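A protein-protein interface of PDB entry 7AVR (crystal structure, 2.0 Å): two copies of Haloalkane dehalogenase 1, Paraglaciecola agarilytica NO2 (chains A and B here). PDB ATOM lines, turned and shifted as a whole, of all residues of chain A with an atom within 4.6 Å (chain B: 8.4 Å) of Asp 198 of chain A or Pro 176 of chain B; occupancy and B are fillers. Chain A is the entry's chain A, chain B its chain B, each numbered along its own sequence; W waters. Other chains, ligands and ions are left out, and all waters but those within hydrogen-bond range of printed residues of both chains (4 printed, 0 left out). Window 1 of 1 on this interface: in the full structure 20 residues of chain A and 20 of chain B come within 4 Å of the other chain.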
ATOM      1  N   ARG A  12      30.914  -5.700   0.891  1.00  0.00           N
ATOM      2  CA  ARG A  12      29.955  -4.823   0.164  1.00  0.00           C
ATOM      3  C   ARG A  12      28.571  -5.414   0.074  1.00  0.00           C
ATOM      4  O   ARG A  12      27.603  -4.669  -0.079  1.00  0.00           O
ATOM      5  CB  ARG A  12      30.486  -4.521  -1.231  1.00  0.00           C
ATOM      6  CG  ARG A  12      31.820  -3.739  -1.288  1.00  0.00           C
ATOM      7  CD  ARG A  12      31.681  -2.329  -0.790  1.00  0.00           C
ATOM      8  NE  ARG A  12      30.978  -1.482  -1.772  1.00  0.00           N
ATOM      9  CZ  ARG A  12      30.865  -0.157  -1.643  1.00  0.00           C
ATOM     10  NH1 ARG A  12      31.419   0.433  -0.561  1.00  0.00           N
ATOM     11  NH2 ARG A  12      30.236   0.529  -2.570  1.00  0.00           N
ATOM     12  N   VAL A 177      25.231   5.759  -9.358  1.00  0.00           N
ATOM     13  CA  VAL A 177      24.462   4.579  -9.686  1.00  0.00           C
ATOM     14  C   VAL A 177      23.151   4.506  -8.913  1.00  0.00           C
ATOM     15  O   VAL A 177      22.076   4.507  -9.521  1.00  0.00           O
ATOM     16  CB  VAL A 177      25.303   3.309  -9.523  1.00  0.00           C
ATOM     17  CG1 VAL A 177      24.472   2.049  -9.646  1.00  0.00           C
ATOM     18  CG2 VAL A 177      26.434   3.314 -10.587  1.00  0.00           C
ATOM     19  N   ALA A 178      23.251   4.560  -7.575  1.00  0.00           N
ATOM     20  CA  ALA A 178      22.062   4.500  -6.724  1.00  0.00           C
ATOM     21  C   ALA A 178      21.147   5.700  -6.968  1.00  0.00           C
ATOM     22  O   ALA A 178      19.932   5.544  -7.025  1.00  0.00           O
ATOM     23  CB  ALA A 178      22.490   4.423  -5.280  1.00  0.00           C
ATOM     24  N   VAL A 191      16.375   3.277   0.770  1.00  0.00           N
ATOM     25  CA  VAL A 191      17.814   3.508   0.941  1.00  0.00           C
ATOM     26  C   VAL A 191      18.587   2.211   1.033  1.00  0.00           C
ATOM     27  O   VAL A 191      19.765   2.179   0.628  1.00  0.00           O
ATOM     28  CB  VAL A 191      18.135   4.468   2.104  1.00  0.00           C
ATOM     29  CG1 VAL A 191      17.781   3.869   3.429  1.00  0.00           C
ATOM     30  CG2 VAL A 191      19.576   4.930   2.015  1.00  0.00           C
ATOM     31  N   ALA A 194      19.237   1.492  -2.513  1.00  0.00           N
ATOM     32  CA  ALA A 194      20.288   2.377  -2.960  1.00  0.00           C
ATOM     33  C   ALA A 194      21.654   1.816  -2.556  1.00  0.00           C
ATOM     34  O   ALA A 194      22.586   1.842  -3.360  1.00  0.00           O
ATOM     35  CB  ALA A 194      20.093   3.763  -2.363  1.00  0.00           C
ATOM     36  N   LEU A 195      21.759   1.276  -1.337  1.00  0.00           N
ATOM     37  CA  LEU A 195      22.953   0.619  -0.853  1.00  0.00           C
ATOM     38  C   LEU A 195      23.337  -0.567  -1.729  1.00  0.00           C
ATOM     39  O   LEU A 195      24.509  -0.705  -2.086  1.00  0.00           O
ATOM     40  CB  LEU A 195      22.761   0.169   0.616  1.00  0.00           C
ATOM     41  CG  LEU A 195      23.927  -0.526   1.308  1.00  0.00           C
ATOM     42  CD1 LEU A 195      24.962   0.565   1.719  1.00  0.00           C
ATOM     43  CD2 LEU A 195      23.327  -1.297   2.532  1.00  0.00           C
ATOM     44  N   ALA A 196      22.350  -1.379  -2.100  1.00  0.00           N
ATOM     45  CA  ALA A 196      22.549  -2.513  -2.990  1.00  0.00           C
ATOM     46  C   ALA A 196      23.027  -2.122  -4.356  1.00  0.00           C
ATOM     47  O   ALA A 196      23.899  -2.806  -4.898  1.00  0.00           O
ATOM     48  CB  ALA A 196      21.292  -3.340  -3.094  1.00  0.00           C
ATOM     49  N   TYR A 197      22.493  -1.045  -4.910  1.00  0.00           N
ATOM     50  CA  TYR A 197      22.900  -0.567  -6.239  1.00  0.00           C
ATOM     51  C   TYR A 197      24.279   0.063  -6.229  1.00  0.00           C
ATOM     52  O   TYR A 197      25.025  -0.150  -7.184  1.00  0.00           O
ATOM     53  CB  TYR A 197      21.806   0.370  -6.830  1.00  0.00           C
ATOM     54  CG  TYR A 197      20.620  -0.405  -7.382  1.00  0.00           C
ATOM     55  CD1 TYR A 197      20.778  -1.273  -8.483  1.00  0.00           C
ATOM     56  CD2 TYR A 197      19.347  -0.209  -6.885  1.00  0.00           C
ATOM     57  CE1 TYR A 197      19.682  -2.007  -8.966  1.00  0.00           C
ATOM     58  CE2 TYR A 197      18.256  -0.960  -7.384  1.00  0.00           C
ATOM     59  CZ  TYR A 197      18.423  -1.808  -8.413  1.00  0.00           C
ATOM     60  OH  TYR A 197      17.347  -2.456  -8.906  1.00  0.00           O
ATOM     61  N   ASP A 198      24.667   0.747  -5.160  1.00  0.00           N
ATOM     62  CA  ASP A 198      26.057   1.273  -5.004  1.00  0.00           C
ATOM     63  C   ASP A 198      27.053   0.184  -4.606  1.00  0.00           C
ATOM     64  O   ASP A 198      28.256   0.409  -4.782  1.00  0.00           O
ATOM     65  CB  ASP A 198      26.105   2.408  -3.996  1.00  0.00           C
ATOM     66  CG  ASP A 198      25.877   3.808  -4.609  1.00  0.00           C
ATOM     67  OD1 ASP A 198      25.601   3.874  -5.821  1.00  0.00           O
ATOM     68  OD2 ASP A 198      25.925   4.767  -3.794  1.00  0.00           O
ATOM     69  N   ALA A 199      26.562  -0.955  -4.079  1.00  0.00           N
ATOM     70  CA  ALA A 199      27.436  -2.026  -3.465  1.00  0.00           C
ATOM     71  C   ALA A 199      28.544  -2.547  -4.392  1.00  0.00           C
ATOM     72  O   ALA A 199      29.669  -2.719  -3.948  1.00  0.00           O
ATOM     73  CB  ALA A 199      26.636  -3.167  -2.890  1.00  0.00           C
ATOM     74  N   PRO A 200      28.259  -2.751  -5.705  1.00  0.00           N
ATOM     75  CA  PRO A 200      29.347  -3.255  -6.567  1.00  0.00           C
ATOM     76  C   PRO A 200      30.554  -2.349  -6.719  1.00  0.00           C
ATOM     77  O   PRO A 200      31.607  -2.833  -7.137  1.00  0.00           O
ATOM     78  CB  PRO A 200      28.638  -3.465  -7.929  1.00  0.00           C
ATOM     79  CG  PRO A 200      27.188  -3.633  -7.561  1.00  0.00           C
ATOM     80  CD  PRO A 200      26.999  -2.625  -6.449  1.00  0.00           C
ATOM     81  N   PHE A 201      30.437  -1.069  -6.383  1.00  0.00           N
ATOM     82  CA  PHE A 201      31.363   0.012  -6.864  1.00  0.00           C
ATOM     83  C   PHE A 201      31.903   0.865  -5.701  1.00  0.00           C
ATOM     84  O   PHE A 201      31.442   1.983  -5.469  1.00  0.00           O
ATOM     85  CB  PHE A 201      30.646   0.904  -7.907  1.00  0.00           C
ATOM     86  CG  PHE A 201      29.956   0.145  -9.005  1.00  0.00           C
ATOM     87  CD1 PHE A 201      30.694  -0.635  -9.906  1.00  0.00           C
ATOM     88  CD2 PHE A 201      28.562   0.194  -9.137  1.00  0.00           C
ATOM     89  CE1 PHE A 201      30.057  -1.361 -10.910  1.00  0.00           C
ATOM     90  CE2 PHE A 201      27.921  -0.534 -10.166  1.00  0.00           C
ATOM     91  CZ  PHE A 201      28.672  -1.323 -11.051  1.00  0.00           C
ATOM     92  N   PRO B  58      23.470  14.056   4.937  1.00  0.00           N
ATOM     93  CA  PRO B  58      24.857  14.075   4.439  1.00  0.00           C
ATOM     94  C   PRO B  58      24.983  15.027   3.265  1.00  0.00           C
ATOM     95  O   PRO B  58      25.384  14.623   2.161  1.00  0.00           O
ATOM     96  CB  PRO B  58      25.016  12.601   3.998  1.00  0.00           C
ATOM     97  CG  PRO B  58      23.725  12.276   3.415  1.00  0.00           C
ATOM     98  CD  PRO B  58      22.684  13.093   4.170  1.00  0.00           C
ATOM     99  N   TRP B 165      18.301   3.985  12.675  1.00  0.00           N
ATOM    100  CA  TRP B 165      19.177   4.840  11.836  1.00  0.00           C
ATOM    101  C   TRP B 165      20.652   4.716  12.251  1.00  0.00           C
ATOM    102  O   TRP B 165      21.506   4.556  11.396  1.00  0.00           O
ATOM    103  CB  TRP B 165      18.708   6.284  11.838  1.00  0.00           C
ATOM    104  CG  TRP B 165      19.651   7.293  11.233  1.00  0.00           C
ATOM    105  CD1 TRP B 165      20.334   8.289  11.903  1.00  0.00           C
ATOM    106  CD2 TRP B 165      19.990   7.462   9.851  1.00  0.00           C
ATOM    107  NE1 TRP B 165      21.112   8.996  11.012  1.00  0.00           N
ATOM    108  CE2 TRP B 165      20.868   8.554   9.757  1.00  0.00           C
ATOM    109  CE3 TRP B 165      19.641   6.768   8.677  1.00  0.00           C
ATOM    110  CZ2 TRP B 165      21.407   8.974   8.545  1.00  0.00           C
ATOM    111  CZ3 TRP B 165      20.140   7.216   7.460  1.00  0.00           C
ATOM    112  CH2 TRP B 165      21.050   8.262   7.397  1.00  0.00           C
ATOM    113  N   PHE B 168      21.858   1.089  11.387  1.00  0.00           N
ATOM    114  CA  PHE B 168      22.022   1.062   9.890  1.00  0.00           C
ATOM    115  C   PHE B 168      23.377   1.596   9.472  1.00  0.00           C
ATOM    116  O   PHE B 168      24.156   0.894   8.787  1.00  0.00           O
ATOM    117  CB  PHE B 168      20.851   1.841   9.228  1.00  0.00           C
ATOM    118  CG  PHE B 168      20.927   1.932   7.747  1.00  0.00           C
ATOM    119  CD1 PHE B 168      20.824   0.780   6.949  1.00  0.00           C
ATOM    120  CD2 PHE B 168      21.089   3.165   7.105  1.00  0.00           C
ATOM    121  CE1 PHE B 168      20.901   0.877   5.560  1.00  0.00           C
ATOM    122  CE2 PHE B 168      21.179   3.253   5.712  1.00  0.00           C
ATOM    123  CZ  PHE B 168      21.069   2.127   4.954  1.00  0.00           C
ATOM    124  N   ASN B 169      23.708   2.804   9.918  1.00  0.00           N
ATOM    125  CA  ASN B 169      24.979   3.444   9.575  1.00  0.00           C
ATOM    126  C   ASN B 169      26.172   2.720  10.109  1.00  0.00           C
ATOM    127  O   ASN B 169      27.222   2.747   9.481  1.00  0.00           O
ATOM    128  CB  ASN B 169      24.983   4.927   9.985  1.00  0.00           C
ATOM    129  CG  ASN B 169      24.231   5.787   8.997  1.00  0.00           C
ATOM    130  OD1 ASN B 169      24.743   6.170   7.921  1.00  0.00           O
ATOM    131  ND2 ASN B 169      22.997   6.125   9.331  1.00  0.00           N
ATOM    132  N   ILE B 172      26.295  -0.891   7.586  1.00  0.00           N
ATOM    133  CA  ILE B 172      26.661  -0.712   6.183  1.00  0.00           C
ATOM    134  C   ILE B 172      28.137  -0.380   5.914  1.00  0.00           C
ATOM    135  O   ILE B 172      28.847   0.154   6.774  1.00  0.00           O
ATOM    136  CB  ILE B 172      25.740   0.330   5.496  1.00  0.00           C
ATOM    137  CG1 ILE B 172      25.988   1.759   6.086  1.00  0.00           C
ATOM    138  CG2 ILE B 172      24.287  -0.134   5.568  1.00  0.00           C
ATOM    139  CD1 ILE B 172      24.990   2.809   5.645  1.00  0.00           C
ATOM    140  N   SER B 173      28.577  -0.649   4.679  1.00  0.00           N
ATOM    141  CA  SER B 173      29.944  -0.285   4.256  1.00  0.00           C
ATOM    142  C   SER B 173      30.144   1.222   4.301  1.00  0.00           C
ATOM    143  O   SER B 173      31.166   1.700   4.747  1.00  0.00           O
ATOM    144  CB  SER B 173      30.234  -0.868   2.866  1.00  0.00           C
ATOM    145  OG  SER B 173      30.000  -2.276   2.887  1.00  0.00           O
ATOM    146  N   GLU B 174      29.177   1.947   3.755  1.00  0.00           N
ATOM    147  CA  GLU B 174      29.178   3.414   3.748  1.00  0.00           C
ATOM    148  C   GLU B 174      27.797   3.838   3.333  1.00  0.00           C
ATOM    149  O   GLU B 174      27.068   3.024   2.677  1.00  0.00           O
ATOM    150  CB  GLU B 174      30.194   3.941   2.722  1.00  0.00           C
ATOM    151  CG  GLU B 174      29.948   3.679   1.252  1.00  0.00           C
ATOM    152  CD  GLU B 174      31.111   4.028   0.349  1.00  0.00           C
ATOM    153  OE1 GLU B 174      31.336   5.213  -0.012  1.00  0.00           O
ATOM    154  OE2 GLU B 174      31.801   3.046  -0.036  1.00  0.00           O
ATOM    155  N   LEU B 175      27.411   5.054   3.648  1.00  0.00           N
ATOM    156  CA  LEU B 175      26.071   5.540   3.326  1.00  0.00           C
ATOM    157  C   LEU B 175      26.024   5.982   1.836  1.00  0.00           C
ATOM    158  O   LEU B 175      26.885   6.709   1.405  1.00  0.00           O
ATOM    159  CB  LEU B 175      25.716   6.738   4.248  1.00  0.00           C
ATOM    160  CG  LEU B 175      24.340   7.378   4.148  1.00  0.00           C
ATOM    161  CD1 LEU B 175      23.315   6.434   4.705  1.00  0.00           C
ATOM    162  CD2 LEU B 175      24.339   8.725   4.870  1.00  0.00           C
ATOM    163  N   PRO B 176      25.025   5.523   1.059  1.00  0.00           N
ATOM    164  CA  PRO B 176      24.848   5.997  -0.323  1.00  0.00           C
ATOM    165  C   PRO B 176      24.213   7.405  -0.285  1.00  0.00           C
ATOM    166  O   PRO B 176      23.030   7.519  -0.061  1.00  0.00           O
ATOM    167  CB  PRO B 176      23.916   4.913  -0.885  1.00  0.00           C
ATOM    168  CG  PRO B 176      23.141   4.396   0.249  1.00  0.00           C
ATOM    169  CD  PRO B 176      23.968   4.552   1.434  1.00  0.00           C
ATOM    170  N   VAL B 177      25.013   8.442  -0.414  1.00  0.00           N
ATOM    171  CA  VAL B 177      24.628   9.823  -0.139  1.00  0.00           C
ATOM    172  C   VAL B 177      23.537  10.339  -1.102  1.00  0.00           C
ATOM    173  O   VAL B 177      22.452  10.645  -0.656  1.00  0.00           O
ATOM    174  CB  VAL B 177      25.867  10.730  -0.147  1.00  0.00           C
ATOM    175  CG1 VAL B 177      25.522  12.201  -0.145  1.00  0.00           C
ATOM    176  CG2 VAL B 177      26.771  10.367   1.033  1.00  0.00           C
ATOM    177  N   ALA B 178      23.788  10.267  -2.378  1.00  0.00           N
ATOM    178  CA  ALA B 178      22.786  10.629  -3.426  1.00  0.00           C
ATOM    179  C   ALA B 178      21.553   9.767  -3.336  1.00  0.00           C
ATOM    180  O   ALA B 178      20.442  10.273  -3.450  1.00  0.00           O
ATOM    181  CB  ALA B 178      23.429  10.599  -4.815  1.00  0.00           C
ATOM    182  N   GLY B 179      21.755   8.475  -3.128  1.00  0.00           N
ATOM    183  CA  GLY B 179      20.673   7.481  -2.949  1.00  0.00           C
ATOM    184  C   GLY B 179      19.713   7.926  -1.830  1.00  0.00           C
ATOM    185  O   GLY B 179      18.483   7.905  -2.023  1.00  0.00           O
ATOM    186  N   LEU B 180      20.273   8.277  -0.678  1.00  0.00           N
ATOM    187  CA  LEU B 180      19.492   8.662   0.483  1.00  0.00           C
ATOM    188  C   LEU B 180      18.661   9.899   0.199  1.00  0.00           C
ATOM    189  O   LEU B 180      17.457   9.916   0.451  1.00  0.00           O
ATOM    190  CB  LEU B 180      20.415   8.953   1.692  1.00  0.00           C
ATOM    191  CG  LEU B 180      19.667   9.412   2.906  1.00  0.00           C
ATOM    192  CD1 LEU B 180      19.157   8.301   3.710  1.00  0.00           C
ATOM    193  CD2 LEU B 180      20.556  10.310   3.785  1.00  0.00           C
ATOM    194  N   VAL B 181      19.298  10.933  -0.379  1.00  0.00           N
ATOM    195  CA  VAL B 181      18.625  12.200  -0.653  1.00  0.00           C
ATOM    196  C   VAL B 181      17.530  11.996  -1.692  1.00  0.00           C
ATOM    197  O   VAL B 181      16.397  12.543  -1.523  1.00  0.00           O
ATOM    198  CB  VAL B 181      19.589  13.313  -1.071  1.00  0.00           C
ATOM    199  CG1 VAL B 181      18.842  14.605  -1.386  1.00  0.00           C
ATOM    200  CG2 VAL B 181      20.613  13.602   0.056  1.00  0.00           C
ATOM    201  N   ALA B 182      17.851  11.249  -2.755  1.00  0.00           N
ATOM    202  CA  ALA B 182      16.853  10.956  -3.838  1.00  0.00           C
ATOM    203  C   ALA B 182      15.633  10.149  -3.291  1.00  0.00           C
ATOM    204  O   ALA B 182      14.509  10.461  -3.616  1.00  0.00           O
ATOM    205  CB  ALA B 182      17.515  10.293  -5.012  1.00  0.00           C
ATOM    206  N   CYS B 183      15.889   9.157  -2.433  1.00  0.00           N
ATOM    207  CA  CYS B 183      14.844   8.383  -1.791  1.00  0.00           C
ATOM    208  C   CYS B 183      13.938   9.268  -0.969  1.00  0.00           C
ATOM    209  O   CYS B 183      12.708   9.094  -0.992  1.00  0.00           O
ATOM    210  CB  CYS B 183      15.388   7.245  -0.935  1.00  0.00           C
ATOM    211  SG  CYS B 183      16.064   5.903  -1.863  1.00  0.00           S
ATOM    212  N   TYR B 197      25.206  15.676  -5.095  1.00  0.00           N
ATOM    213  CA  TYR B 197      25.230  15.137  -3.758  1.00  0.00           C
ATOM    214  C   TYR B 197      26.339  14.088  -3.570  1.00  0.00           C
ATOM    215  O   TYR B 197      26.961  14.060  -2.517  1.00  0.00           O
ATOM    216  CB  TYR B 197      23.859  14.623  -3.326  1.00  0.00           C
ATOM    217  CG  TYR B 197      22.891  15.708  -2.921  1.00  0.00           C
ATOM    218  CD1 TYR B 197      23.151  16.496  -1.797  1.00  0.00           C
ATOM    219  CD2 TYR B 197      21.687  15.919  -3.599  1.00  0.00           C
ATOM    220  CE1 TYR B 197      22.288  17.551  -1.413  1.00  0.00           C
ATOM    221  CE2 TYR B 197      20.834  16.959  -3.233  1.00  0.00           C
ATOM    222  CZ  TYR B 197      21.126  17.740  -2.136  1.00  0.00           C
ATOM    223  OH  TYR B 197      20.277  18.720  -1.753  1.00  0.00           O
ATOM    224  N   ASP B 198      26.622  13.295  -4.601  1.00  0.00           N
ATOM    225  CA  ASP B 198      27.774  12.346  -4.548  1.00  0.00           C
ATOM    226  C   ASP B 198      29.106  13.037  -4.804  1.00  0.00           C
ATOM    227  O   ASP B 198      30.142  12.421  -4.454  1.00  0.00           O
ATOM    228  CB  ASP B 198      27.574  11.223  -5.552  1.00  0.00           C
ATOM    229  CG  ASP B 198      26.844   9.986  -4.975  1.00  0.00           C
ATOM    230  OD1 ASP B 198      26.427  10.041  -3.806  1.00  0.00           O
ATOM    231  OD2 ASP B 198      26.778   8.955  -5.644  1.00  0.00           O
ATOM    232  N   PHE B 201      32.457  13.111  -2.549  1.00  0.00           N
ATOM    233  CA  PHE B 201      32.898  11.832  -1.992  1.00  0.00           C
ATOM    234  C   PHE B 201      33.299  10.813  -3.065  1.00  0.00           C
ATOM    235  O   PHE B 201      32.506   9.901  -3.423  1.00  0.00           O
ATOM    236  CB  PHE B 201      31.753  11.231  -1.095  1.00  0.00           C
ATOM    237  CG  PHE B 201      31.254  12.182  -0.054  1.00  0.00           C
ATOM    238  CD1 PHE B 201      32.047  12.676   0.940  1.00  0.00           C
ATOM    239  CD2 PHE B 201      29.894  12.619  -0.099  1.00  0.00           C
ATOM    240  CE1 PHE B 201      31.557  13.613   1.882  1.00  0.00           C
ATOM    241  CE2 PHE B 201      29.398  13.527   0.837  1.00  0.00           C
ATOM    242  CZ  PHE B 201      30.227  14.003   1.839  1.00  0.00           C
ATOM    243  N   LYS B 207      34.389  10.193   3.468  1.00  0.00           N
ATOM    244  CA  LYS B 207      33.076  10.130   4.113  1.00  0.00           C
ATOM    245  C   LYS B 207      33.144   9.961   5.642  1.00  0.00           C
ATOM    246  O   LYS B 207      32.131   9.670   6.269  1.00  0.00           O
ATOM    247  CB  LYS B 207      32.266   8.951   3.523  1.00  0.00           C
ATOM    248  CG  LYS B 207      31.714   9.180   2.144  1.00  0.00           C
ATOM    249  CD  LYS B 207      30.590   8.171   1.837  1.00  0.00           C
ATOM    250  CE  LYS B 207      30.253   8.151   0.357  1.00  0.00           C
ATOM    251  NZ  LYS B 207      29.254   7.066   0.144  1.00  0.00           N
ATOM    252  N   VAL B 210      30.547  12.016   7.255  1.00  0.00           N
ATOM    253  CA  VAL B 210      29.252  11.376   6.940  1.00  0.00           C
ATOM    254  C   VAL B 210      28.989  10.181   7.890  1.00  0.00           C
ATOM    255  O   VAL B 210      27.855   9.984   8.349  1.00  0.00           O
ATOM    256  CB  VAL B 210      29.237  10.849   5.468  1.00  0.00           C
ATOM    257  CG1 VAL B 210      27.995  10.032   5.146  1.00  0.00           C
ATOM    258  CG2 VAL B 210      29.363  12.027   4.479  1.00  0.00           C
HETATM  259  O   HOH W   1      24.563   7.114  -3.651  1.00  0.00           O
HETATM  260  O   HOH W   2      27.669   4.634  -1.556  1.00  0.00           O
HETATM  261  O   HOH W   3      24.567   7.658  -6.698  1.00  0.00           O
HETATM  262  O   HOH W   4      29.877   3.526  -2.693  1.00  0.00           O
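The side-chain sulfur (SG) of Cys 183 of chain B lies within hydrogen-bond range of the backbone NH (N) of Val 191 of chain A (3.7 Å).
The guanidinium group of Arg 12 of chain A lies within salt-bridge range of the side-chain carboxylate of Glu 174 of chain B (2.7 Å).
The side-chain sulfur (SG) of Cys 183 of chain B is in hydrogen-bond range of the backbone carbonyl oxygen (O) of Gly 179 of chain B, at 3.1 Å.
The backbone carbonyl oxygen of Phe 201 of chain A lies within hydrogen-bond range of the guanidinium group of Arg 12 of chain A (3.5 Å).
The guanidinium group (NH2) of Arg 12 of chain A sits at hydrogen-bond distance from the backbone carbonyl oxygen (O) of Asp 198 of chain A, at 3.0 Å.
N of Ala 178 of chain A sits at hydrogen-bond distance from OD1 of Asp 198 of chain A, 3.0 Å away.
The backbone carbonyl oxygen of Ala 199 of chain A lies within hydrogen-bond range of the guanidinium group of Arg 12 of chain A.
The side-chain carboxylate of Glu 174 of chain B is in salt-bridge range of the side-chain amino group of Lys 207 of chain B, at 2.8 Å.
Arg 12 of chain A touches Ser 173 of chain B (CA to OG, 3.7 Å).
Leu 180 of chain B touches Val 191 of chain A.
CA of Gly 179 of chain B touches CB of Ala 194 of chain A, at 3.8 Å.
Leu 195 of chain A touches Ile 172 of chain B (CD2 to CG2, 3.4 Å).
CD1 of Leu 195 of chain A touches O of Glu 174 of chain B (3.4 Å).
CG of Pro 176 of chain B touches N of Leu 195 of chain A (3.8 Å).
CB of Pro 176 of chain B touches OD2 of Asp 198 of chain A, at 3.5 Å.
Asp 198 of chain A touches one residue of chain B.
Of the printed residues of chain A, Pro 176 of chain B touches Leu 195 and Asp 198.
No residue of chain B comes within 4 Å of Ala 199 of chain A.
Of the printed residues of chain B, Val 191 of chain A touches Leu 180 and Cys 183.
Printed residues of chain A within 4 Å of Glu 174 of chain B: Arg 12 and Leu 195.
Printed residues of chain B within 4 Å of Leu 195 of chain A: Ile 172, Glu 174 and Pro 176.
Of the printed residues of chain A, Gly 179 of chain B touches Ala 194 (3.8 Å).
Tyr 197 of chain A touches none of the printed residues of chain B.
Asn 169 of chain B touches none of the printed residues of chain A.
The nearest residue of chain B that does not touch Asp 198 of chain A is Asp 198 of chain B (4.7 Å).
Of the 21 printed residues of chain B, 7 touch a printed residue of chain A.
Printed residues of chain B that touch a printed residue of chain A: Ile 172, Ser 173, Glu 174, Pro 176, Gly 179, Leu 180 and Cys 183.
Hydrophobic or aromatic side chains of chain A that line the printed part of chain B: Val 191, Ala 194 and Leu 195.
Among the printed residues, Asp or Glu carboxylates within 4 Å of a Lys or Arg side-chain nitrogen of the other chain: Arg 12 of chain A with Glu 174 of chain B (2.7 Å).
5 positions are printed for both chains.
Of the 9 pairs that touch across the chains among the printed residues, none has its exchanged pair printed and touching as well.
Water W1 lies within hydrogen-bond range of OD2 of Asp 198 of chain A (2.7 Å), N of Gly 179 of chain B (3.2 Å), OD1 of Asp 198 of chain B (3.5 Å) and N of Ala 178 of chain B (3.5 Å).
Water W3 lies within hydrogen-bond range of OD2 of Asp 198 of chain B (2.8 Å), N of Val 177 of chain A (3.3 Å) and N of Ala 178 of chain A (3.5 Å).
Water W2 lies within hydrogen-bond range of OD2 of Asp 198 of chain A (2.8 Å) and NZ of Lys 207 of chain B (3.4 Å).
Water W4 lies within hydrogen-bond range of the guanidinium group of Arg 12 of chain A and the side-chain carboxylate of Glu 174 of chain B.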
